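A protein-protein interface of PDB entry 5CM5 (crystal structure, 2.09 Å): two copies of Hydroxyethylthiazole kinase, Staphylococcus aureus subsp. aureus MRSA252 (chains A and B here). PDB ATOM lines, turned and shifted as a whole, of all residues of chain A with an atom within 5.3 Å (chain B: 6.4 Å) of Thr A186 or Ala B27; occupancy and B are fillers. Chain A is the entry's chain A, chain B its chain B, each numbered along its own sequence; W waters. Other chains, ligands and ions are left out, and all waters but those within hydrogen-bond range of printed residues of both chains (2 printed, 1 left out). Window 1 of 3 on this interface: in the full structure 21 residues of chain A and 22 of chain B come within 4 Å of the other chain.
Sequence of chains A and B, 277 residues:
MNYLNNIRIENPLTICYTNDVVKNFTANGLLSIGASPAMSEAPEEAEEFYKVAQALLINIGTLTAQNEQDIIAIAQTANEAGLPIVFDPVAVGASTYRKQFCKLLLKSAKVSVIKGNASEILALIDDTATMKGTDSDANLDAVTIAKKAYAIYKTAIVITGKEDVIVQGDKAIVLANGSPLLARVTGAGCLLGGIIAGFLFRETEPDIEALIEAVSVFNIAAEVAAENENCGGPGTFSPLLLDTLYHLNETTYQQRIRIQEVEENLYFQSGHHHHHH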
ATOM      1  N   VAL A  21       7.605 -26.967  -4.837  1.00  0.00           N
ATOM      2  CA  VAL A  21       6.267 -26.998  -5.316  1.00  0.00           C
ATOM      3  C   VAL A  21       5.973 -25.728  -6.155  1.00  0.00           C
ATOM      4  O   VAL A  21       5.087 -25.741  -6.971  1.00  0.00           O
ATOM      5  CB  VAL A  21       5.268 -27.176  -4.152  1.00  0.00           C
ATOM      6  CG1 VAL A  21       3.853 -27.341  -4.617  1.00  0.00           C
ATOM      7  CG2 VAL A  21       5.617 -28.404  -3.305  1.00  0.00           C
ATOM      8  N   VAL A  22       6.738 -24.655  -5.945  1.00  0.00           N
ATOM      9  CA  VAL A  22       6.367 -23.307  -6.403  1.00  0.00           C
ATOM     10  C   VAL A  22       7.399 -22.586  -7.204  1.00  0.00           C
ATOM     11  O   VAL A  22       7.191 -21.422  -7.549  1.00  0.00           O
ATOM     12  CB  VAL A  22       6.041 -22.385  -5.186  1.00  0.00           C
ATOM     13  CG1 VAL A  22       5.019 -23.060  -4.308  1.00  0.00           C
ATOM     14  CG2 VAL A  22       7.292 -22.097  -4.338  1.00  0.00           C
ATOM     15  N   ARG A 184      -6.806 -21.549  -3.143  1.00  0.00           N
ATOM     16  CA  ARG A 184      -6.932 -22.847  -3.788  1.00  0.00           C
ATOM     17  C   ARG A 184      -5.905 -23.039  -4.876  1.00  0.00           C
ATOM     18  O   ARG A 184      -6.057 -23.930  -5.744  1.00  0.00           O
ATOM     19  CB  ARG A 184      -8.373 -23.008  -4.348  1.00  0.00           C
ATOM     20  CG  ARG A 184      -9.439 -22.958  -3.270  1.00  0.00           C
ATOM     21  CD  ARG A 184      -9.010 -24.108  -2.318  1.00  0.00           C
ATOM     22  NE  ARG A 184     -10.021 -24.585  -1.428  1.00  0.00           N
ATOM     23  CZ  ARG A 184     -10.952 -25.474  -1.759  1.00  0.00           C
ATOM     24  NH1 ARG A 184     -11.032 -26.013  -2.990  1.00  0.00           N
ATOM     25  NH2 ARG A 184     -11.830 -25.807  -0.838  1.00  0.00           N
ATOM     26  N   VAL A 185      -4.924 -22.148  -4.900  1.00  0.00           N
ATOM     27  CA  VAL A 185      -3.842 -22.229  -5.830  1.00  0.00           C
ATOM     28  C   VAL A 185      -2.559 -22.399  -5.018  1.00  0.00           C
ATOM     29  O   VAL A 185      -2.260 -21.560  -4.187  1.00  0.00           O
ATOM     30  CB  VAL A 185      -3.757 -20.978  -6.697  1.00  0.00           C
ATOM     31  CG1 VAL A 185      -2.522 -21.052  -7.616  1.00  0.00           C
ATOM     32  CG2 VAL A 185      -5.027 -20.824  -7.537  1.00  0.00           C
ATOM     33  N   THR A 186      -1.806 -23.480  -5.272  1.00  0.00           N
ATOM     34  CA  THR A 186      -0.673 -23.820  -4.391  1.00  0.00           C
ATOM     35  C   THR A 186       0.435 -22.809  -4.400  1.00  0.00           C
ATOM     36  O   THR A 186       1.076 -22.536  -3.344  1.00  0.00           O
ATOM     37  CB  THR A 186      -0.100 -25.265  -4.544  1.00  0.00           C
ATOM     38  OG1 THR A 186       0.772 -25.558  -3.421  1.00  0.00           O
ATOM     39  CG2 THR A 186       0.673 -25.453  -5.804  1.00  0.00           C
ATOM     40  N   GLY A 187       0.752 -22.189  -5.518  1.00  0.00           N
ATOM     41  CA  GLY A 187       1.848 -21.163  -5.294  1.00  0.00           C
ATOM     42  C   GLY A 187       1.594 -19.886  -4.412  1.00  0.00           C
ATOM     43  O   GLY A 187       2.548 -19.224  -3.988  1.00  0.00           O
ATOM     44  N   ALA A 188       0.328 -19.520  -4.176  1.00  0.00           N
ATOM     45  CA  ALA A 188      -0.051 -18.080  -4.023  1.00  0.00           C
ATOM     46  C   ALA A 188       0.816 -17.289  -3.061  1.00  0.00           C
ATOM     47  O   ALA A 188       1.502 -16.340  -3.481  1.00  0.00           O
ATOM     48  CB  ALA A 188      -1.507 -17.939  -3.639  1.00  0.00           C
ATOM     49  N   GLY A 189       0.829 -17.688  -1.799  1.00  0.00           N
ATOM     50  CA  GLY A 189       1.572 -16.941  -0.810  1.00  0.00           C
ATOM     51  C   GLY A 189       3.067 -17.079  -0.992  1.00  0.00           C
ATOM     52  O   GLY A 189       3.866 -16.169  -0.659  1.00  0.00           O
ATOM     53  N   CYS A 190       3.477 -18.213  -1.544  1.00  0.00           N
ATOM     54  CA  CYS A 190       4.892 -18.436  -1.749  1.00  0.00           C
ATOM     55  C   CYS A 190       5.301 -17.465  -2.886  1.00  0.00           C
ATOM     56  O   CYS A 190       6.351 -16.765  -2.832  1.00  0.00           O
ATOM     57  CB  CYS A 190       5.153 -19.989  -1.955  1.00  0.00           C
ATOM     58  SG  CYS A 190       4.651 -21.198  -0.614  1.00  0.00           S
ATOM     59  N   CYS B  16       2.680 -35.593   0.712  1.00  0.00           N
ATOM     60  CA  CYS B  16       3.161 -36.133  -0.543  1.00  0.00           C
ATOM     61  C   CYS B  16       4.674 -36.094  -0.639  1.00  0.00           C
ATOM     62  O   CYS B  16       5.274 -35.006  -0.655  1.00  0.00           O
ATOM     63  CB  CYS B  16       2.577 -35.327  -1.769  1.00  0.00           C
ATOM     64  SG  CYS B  16       0.814 -35.342  -1.809  1.00  0.00           S
ATOM     65  N   VAL B  22       5.976 -33.396 -10.980  1.00  0.00           N
ATOM     66  CA  VAL B  22       4.523 -33.355 -10.722  1.00  0.00           C
ATOM     67  C   VAL B  22       4.118 -32.723  -9.402  1.00  0.00           C
ATOM     68  O   VAL B  22       2.948 -32.794  -9.027  1.00  0.00           O
ATOM     69  CB  VAL B  22       3.930 -34.779 -10.745  1.00  0.00           C
ATOM     70  CG1 VAL B  22       4.313 -35.418 -12.029  1.00  0.00           C
ATOM     71  CG2 VAL B  22       4.445 -35.632  -9.572  1.00  0.00           C
ATOM     72  N   LYS B  23       5.068 -32.170  -8.644  1.00  0.00           N
ATOM     73  CA  LYS B  23       4.699 -31.717  -7.305  1.00  0.00           C
ATOM     74  C   LYS B  23       3.618 -30.652  -7.373  1.00  0.00           C
ATOM     75  O   LYS B  23       2.671 -30.680  -6.626  1.00  0.00           O
ATOM     76  CB  LYS B  23       5.910 -31.131  -6.579  1.00  0.00           C
ATOM     77  CG  LYS B  23       6.768 -32.206  -5.941  1.00  0.00           C
ATOM     78  CD  LYS B  23       8.062 -31.687  -5.341  1.00  0.00           C
ATOM     79  CE  LYS B  23       8.990 -32.875  -5.226  1.00  0.00           C
ATOM     80  NZ  LYS B  23      10.222 -32.510  -4.504  1.00  0.00           N
ATOM     81  N   ASN B  24       3.853 -29.648  -8.197  1.00  0.00           N
ATOM     82  CA  ASN B  24       2.924 -28.539  -8.258  1.00  0.00           C
ATOM     83  C   ASN B  24       1.542 -29.021  -8.670  1.00  0.00           C
ATOM     84  O   ASN B  24       0.522 -28.533  -8.152  1.00  0.00           O
ATOM     85  CB  ASN B  24       3.444 -27.460  -9.190  1.00  0.00           C
ATOM     86  CG  ASN B  24       2.442 -26.379  -9.425  1.00  0.00           C
ATOM     87  OD1 ASN B  24       1.610 -26.439 -10.416  1.00  0.00           O
ATOM     88  ND2 ASN B  24       2.503 -25.352  -8.620  1.00  0.00           N
ATOM     89  N   PHE B  25       1.486 -29.895  -9.664  1.00  0.00           N
ATOM     90  CA  PHE B  25       0.187 -30.331 -10.209  1.00  0.00           C
ATOM     91  C   PHE B  25      -0.539 -31.181  -9.198  1.00  0.00           C
ATOM     92  O   PHE B  25      -1.756 -31.122  -9.051  1.00  0.00           O
ATOM     93  CB  PHE B  25       0.458 -31.069 -11.491  1.00  0.00           C
ATOM     94  CG  PHE B  25      -0.752 -31.351 -12.331  1.00  0.00           C
ATOM     95  CD1 PHE B  25      -1.648 -30.398 -12.600  1.00  0.00           C
ATOM     96  CD2 PHE B  25      -0.957 -32.632 -12.822  1.00  0.00           C
ATOM     97  CE1 PHE B  25      -2.769 -30.653 -13.420  1.00  0.00           C
ATOM     98  CE2 PHE B  25      -2.042 -32.916 -13.659  1.00  0.00           C
ATOM     99  CZ  PHE B  25      -2.983 -31.933 -13.890  1.00  0.00           C
ATOM    100  N   THR B  26       0.222 -31.991  -8.467  1.00  0.00           N
ATOM    101  CA  THR B  26      -0.352 -32.869  -7.455  1.00  0.00           C
ATOM    102  C   THR B  26      -0.940 -32.012  -6.326  1.00  0.00           C
ATOM    103  O   THR B  26      -2.087 -32.253  -5.883  1.00  0.00           O
ATOM    104  CB  THR B  26       0.731 -33.788  -6.852  1.00  0.00           C
ATOM    105  OG1 THR B  26       1.283 -34.615  -7.878  1.00  0.00           O
ATOM    106  CG2 THR B  26       0.136 -34.665  -5.814  1.00  0.00           C
ATOM    107  N   ALA B  27      -0.177 -31.025  -5.846  1.00  0.00           N
ATOM    108  CA  ALA B  27      -0.699 -30.113  -4.808  1.00  0.00           C
ATOM    109  C   ALA B  27      -1.946 -29.388  -5.297  1.00  0.00           C
ATOM    110  O   ALA B  27      -2.940 -29.259  -4.597  1.00  0.00           O
ATOM    111  CB  ALA B  27       0.333 -29.091  -4.410  1.00  0.00           C
ATOM    112  N   ASN B  28      -1.902 -28.880  -6.510  1.00  0.00           N
ATOM    113  CA  ASN B  28      -3.126 -28.198  -7.058  1.00  0.00           C
ATOM    114  C   ASN B  28      -4.342 -29.121  -7.232  1.00  0.00           C
ATOM    115  O   ASN B  28      -5.477 -28.689  -7.043  1.00  0.00           O
ATOM    116  CB  ASN B  28      -2.795 -27.515  -8.371  1.00  0.00           C
ATOM    117  CG  ASN B  28      -2.112 -26.206  -8.166  1.00  0.00           C
ATOM    118  OD1 ASN B  28      -2.531 -25.406  -7.342  1.00  0.00           O
ATOM    119  ND2 ASN B  28      -1.075 -25.948  -8.922  1.00  0.00           N
ATOM    120  N   GLY B  29      -4.116 -30.369  -7.616  1.00  0.00           N
ATOM    121  CA  GLY B  29      -5.222 -31.354  -7.780  1.00  0.00           C
ATOM    122  C   GLY B  29      -5.855 -31.621  -6.422  1.00  0.00           C
ATOM    123  O   GLY B  29      -7.092 -31.623  -6.269  1.00  0.00           O
ATOM    124  N   LEU B  30      -5.002 -31.811  -5.418  1.00  0.00           N
ATOM    125  CA  LEU B  30      -5.509 -31.959  -4.107  1.00  0.00           C
ATOM    126  C   LEU B  30      -6.264 -30.744  -3.629  1.00  0.00           C
ATOM    127  O   LEU B  30      -7.278 -30.886  -2.941  1.00  0.00           O
ATOM    128  CB  LEU B  30      -4.341 -32.352  -3.112  1.00  0.00           C
ATOM    129  CG  LEU B  30      -3.998 -33.859  -3.240  1.00  0.00           C
ATOM    130  CD1 LEU B  30      -2.659 -34.214  -2.651  1.00  0.00           C
ATOM    131  CD2 LEU B  30      -5.077 -34.757  -2.621  1.00  0.00           C
ATOM    132  N   LEU B  31      -5.696 -29.553  -3.805  1.00  0.00           N
ATOM    133  CA  LEU B  31      -6.364 -28.391  -3.303  1.00  0.00           C
ATOM    134  C   LEU B  31      -7.722 -28.308  -4.024  1.00  0.00           C
ATOM    135  O   LEU B  31      -8.689 -27.866  -3.406  1.00  0.00           O
ATOM    136  CB  LEU B  31      -5.582 -27.080  -3.554  1.00  0.00           C
ATOM    137  CG  LEU B  31      -4.434 -26.769  -2.615  1.00  0.00           C
ATOM    138  CD1 LEU B  31      -3.594 -25.632  -3.204  1.00  0.00           C
ATOM    139  CD2 LEU B  31      -4.911 -26.410  -1.192  1.00  0.00           C
ATOM    140  N   SER B  32      -7.782 -28.668  -5.328  1.00  0.00           N
ATOM    141  CA  SER B  32      -9.036 -28.469  -6.056  1.00  0.00           C
ATOM    142  C   SER B  32     -10.203 -29.322  -5.500  1.00  0.00           C
ATOM    143  O   SER B  32     -11.380 -28.904  -5.533  1.00  0.00           O
ATOM    144  CB  SER B  32      -8.842 -28.633  -7.577  1.00  0.00           C
ATOM    145  OG  SER B  32      -8.706 -30.035  -7.850  1.00  0.00           O
ATOM    146  N   ALA B  35      -8.634 -31.016  -0.457  1.00  0.00           N
ATOM    147  CA  ALA B  35      -7.639 -31.583   0.516  1.00  0.00           C
ATOM    148  C   ALA B  35      -6.602 -30.536   0.854  1.00  0.00           C
ATOM    149  O   ALA B  35      -6.500 -29.505   0.195  1.00  0.00           O
ATOM    150  CB  ALA B  35      -6.995 -32.848  -0.009  1.00  0.00           C
ATOM    151  N   PRO B  37      -2.700 -30.402   0.878  1.00  0.00           N
ATOM    152  CA  PRO B  37      -1.435 -31.065   0.571  1.00  0.00           C
ATOM    153  C   PRO B  37      -0.232 -30.481   1.295  1.00  0.00           C
ATOM    154  O   PRO B  37      -0.184 -29.324   1.540  1.00  0.00           O
ATOM    155  CB  PRO B  37      -1.279 -30.844  -0.922  1.00  0.00           C
ATOM    156  CG  PRO B  37      -1.928 -29.494  -1.114  1.00  0.00           C
ATOM    157  CD  PRO B  37      -3.142 -29.548  -0.214  1.00  0.00           C
ATOM    158  N   MET B  39       3.978 -31.125   0.934  1.00  0.00           N
ATOM    159  CA  MET B  39       5.022 -31.865   0.336  1.00  0.00           C
ATOM    160  C   MET B  39       6.205 -31.845   1.336  1.00  0.00           C
ATOM    161  O   MET B  39       7.254 -31.316   1.033  1.00  0.00           O
ATOM    162  CB  MET B  39       5.469 -31.238  -0.989  1.00  0.00           C
ATOM    163  CG  MET B  39       4.609 -31.687  -2.215  1.00  0.00           C
ATOM    164  SD  MET B  39       2.865 -31.539  -1.900  1.00  0.00           S
ATOM    165  CE  MET B  39       2.277 -32.094  -3.597  1.00  0.00           C
ATOM    166  N   LEU B 191      -0.638 -37.664 -10.276  1.00  0.00           N
ATOM    167  CA  LEU B 191      -1.715 -36.946  -9.590  1.00  0.00           C
ATOM    168  C   LEU B 191      -2.762 -37.910  -9.026  1.00  0.00           C
ATOM    169  O   LEU B 191      -3.238 -37.704  -7.928  1.00  0.00           O
ATOM    170  CB  LEU B 191      -2.342 -35.832 -10.468  1.00  0.00           C
ATOM    171  CG  LEU B 191      -3.659 -35.202  -9.969  1.00  0.00           C
ATOM    172  CD1 LEU B 191      -3.550 -34.643  -8.570  1.00  0.00           C
ATOM    173  CD2 LEU B 191      -4.181 -34.108 -10.908  1.00  0.00           C
HETATM  174  O   HOH W   1       5.302 -23.892  -9.547  1.00  0.00           O
HETATM  175  O   HOH W   2      -6.013 -25.923  -7.767  1.00  0.00           O
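The side-chain amide nitrogen (ND2) of Asn B24 sits at hydrogen-bond distance from the backbone carbonyl oxygen (O) of Val A21, at 3.1 Å.
The backbone carbonyl oxygen (O) of Leu B31 sits at hydrogen-bond distance from the guanidinium group (NH1) of Arg A184 (3.0 Å).
N of Thr A186 is in hydrogen-bond range of OD1 of Asn B28 (2.9 Å).
OD1 of Asn B24 sits at hydrogen-bond distance from ND2 of Asn B28 (3.1 Å).
The side-chain hydroxyl (OG) of Ser B32 sits at hydrogen-bond distance from the backbone carbonyl oxygen (O) of Gly B29 (2.8 Å).
Among the printed residues, merely in contact across the chains: Thr A186 with Asn B24, Thr A186 with Leu B31, Val A21 with Met B39, Thr A186 with Ala B27, Val A185 with Asn B28, Val A185 with Leu B31, Arg A184 with Ser B32 and Val A21 with Ala B27.
Thr A186 touches just these residues of chain B: Asn B24, Ala B27, Asn B28 and Leu B31.
Ala B27 touches just these residues of chain A: Val A21 (3.9 Å) and Thr A186 (3.7 Å).
Of the printed residues of chain A, Met B39 touches Val A21.
Of the printed residues of chain A, Asn B24 touches Val A21 and Thr A186.
The nearest printed residue of chain A that does not touch Ala B27 is Arg A184 (6.3 Å).
The nearest printed residue of chain B that does not touch Val A185 is Asn B24 (6.7 Å).
Of the 9 printed residues of chain A, 4 touch a printed residue of chain B.
Hydrophobic or aromatic side chains of chain A within 4 Å of the printed part of chain B: Val A21.
Among the printed residues, no Asp or Glu carboxylate lies within 4 Å of a Lys or Arg side-chain nitrogen of the other chain.
Position printed for both chains: 22.
Of the 11 pairs that touch across the chains among the printed residues, none has its exchanged pair printed and touching as well.
Water W2 lies within hydrogen-bond range of the backbone carbonyl oxygen (O) of Arg A184 and the backbone carbonyl oxygen (O) of Asn B28.
Water W1 lies within hydrogen-bond range of O of Val A21 (3.2 Å) and ND2 of Asn B24 (3.3 Å).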
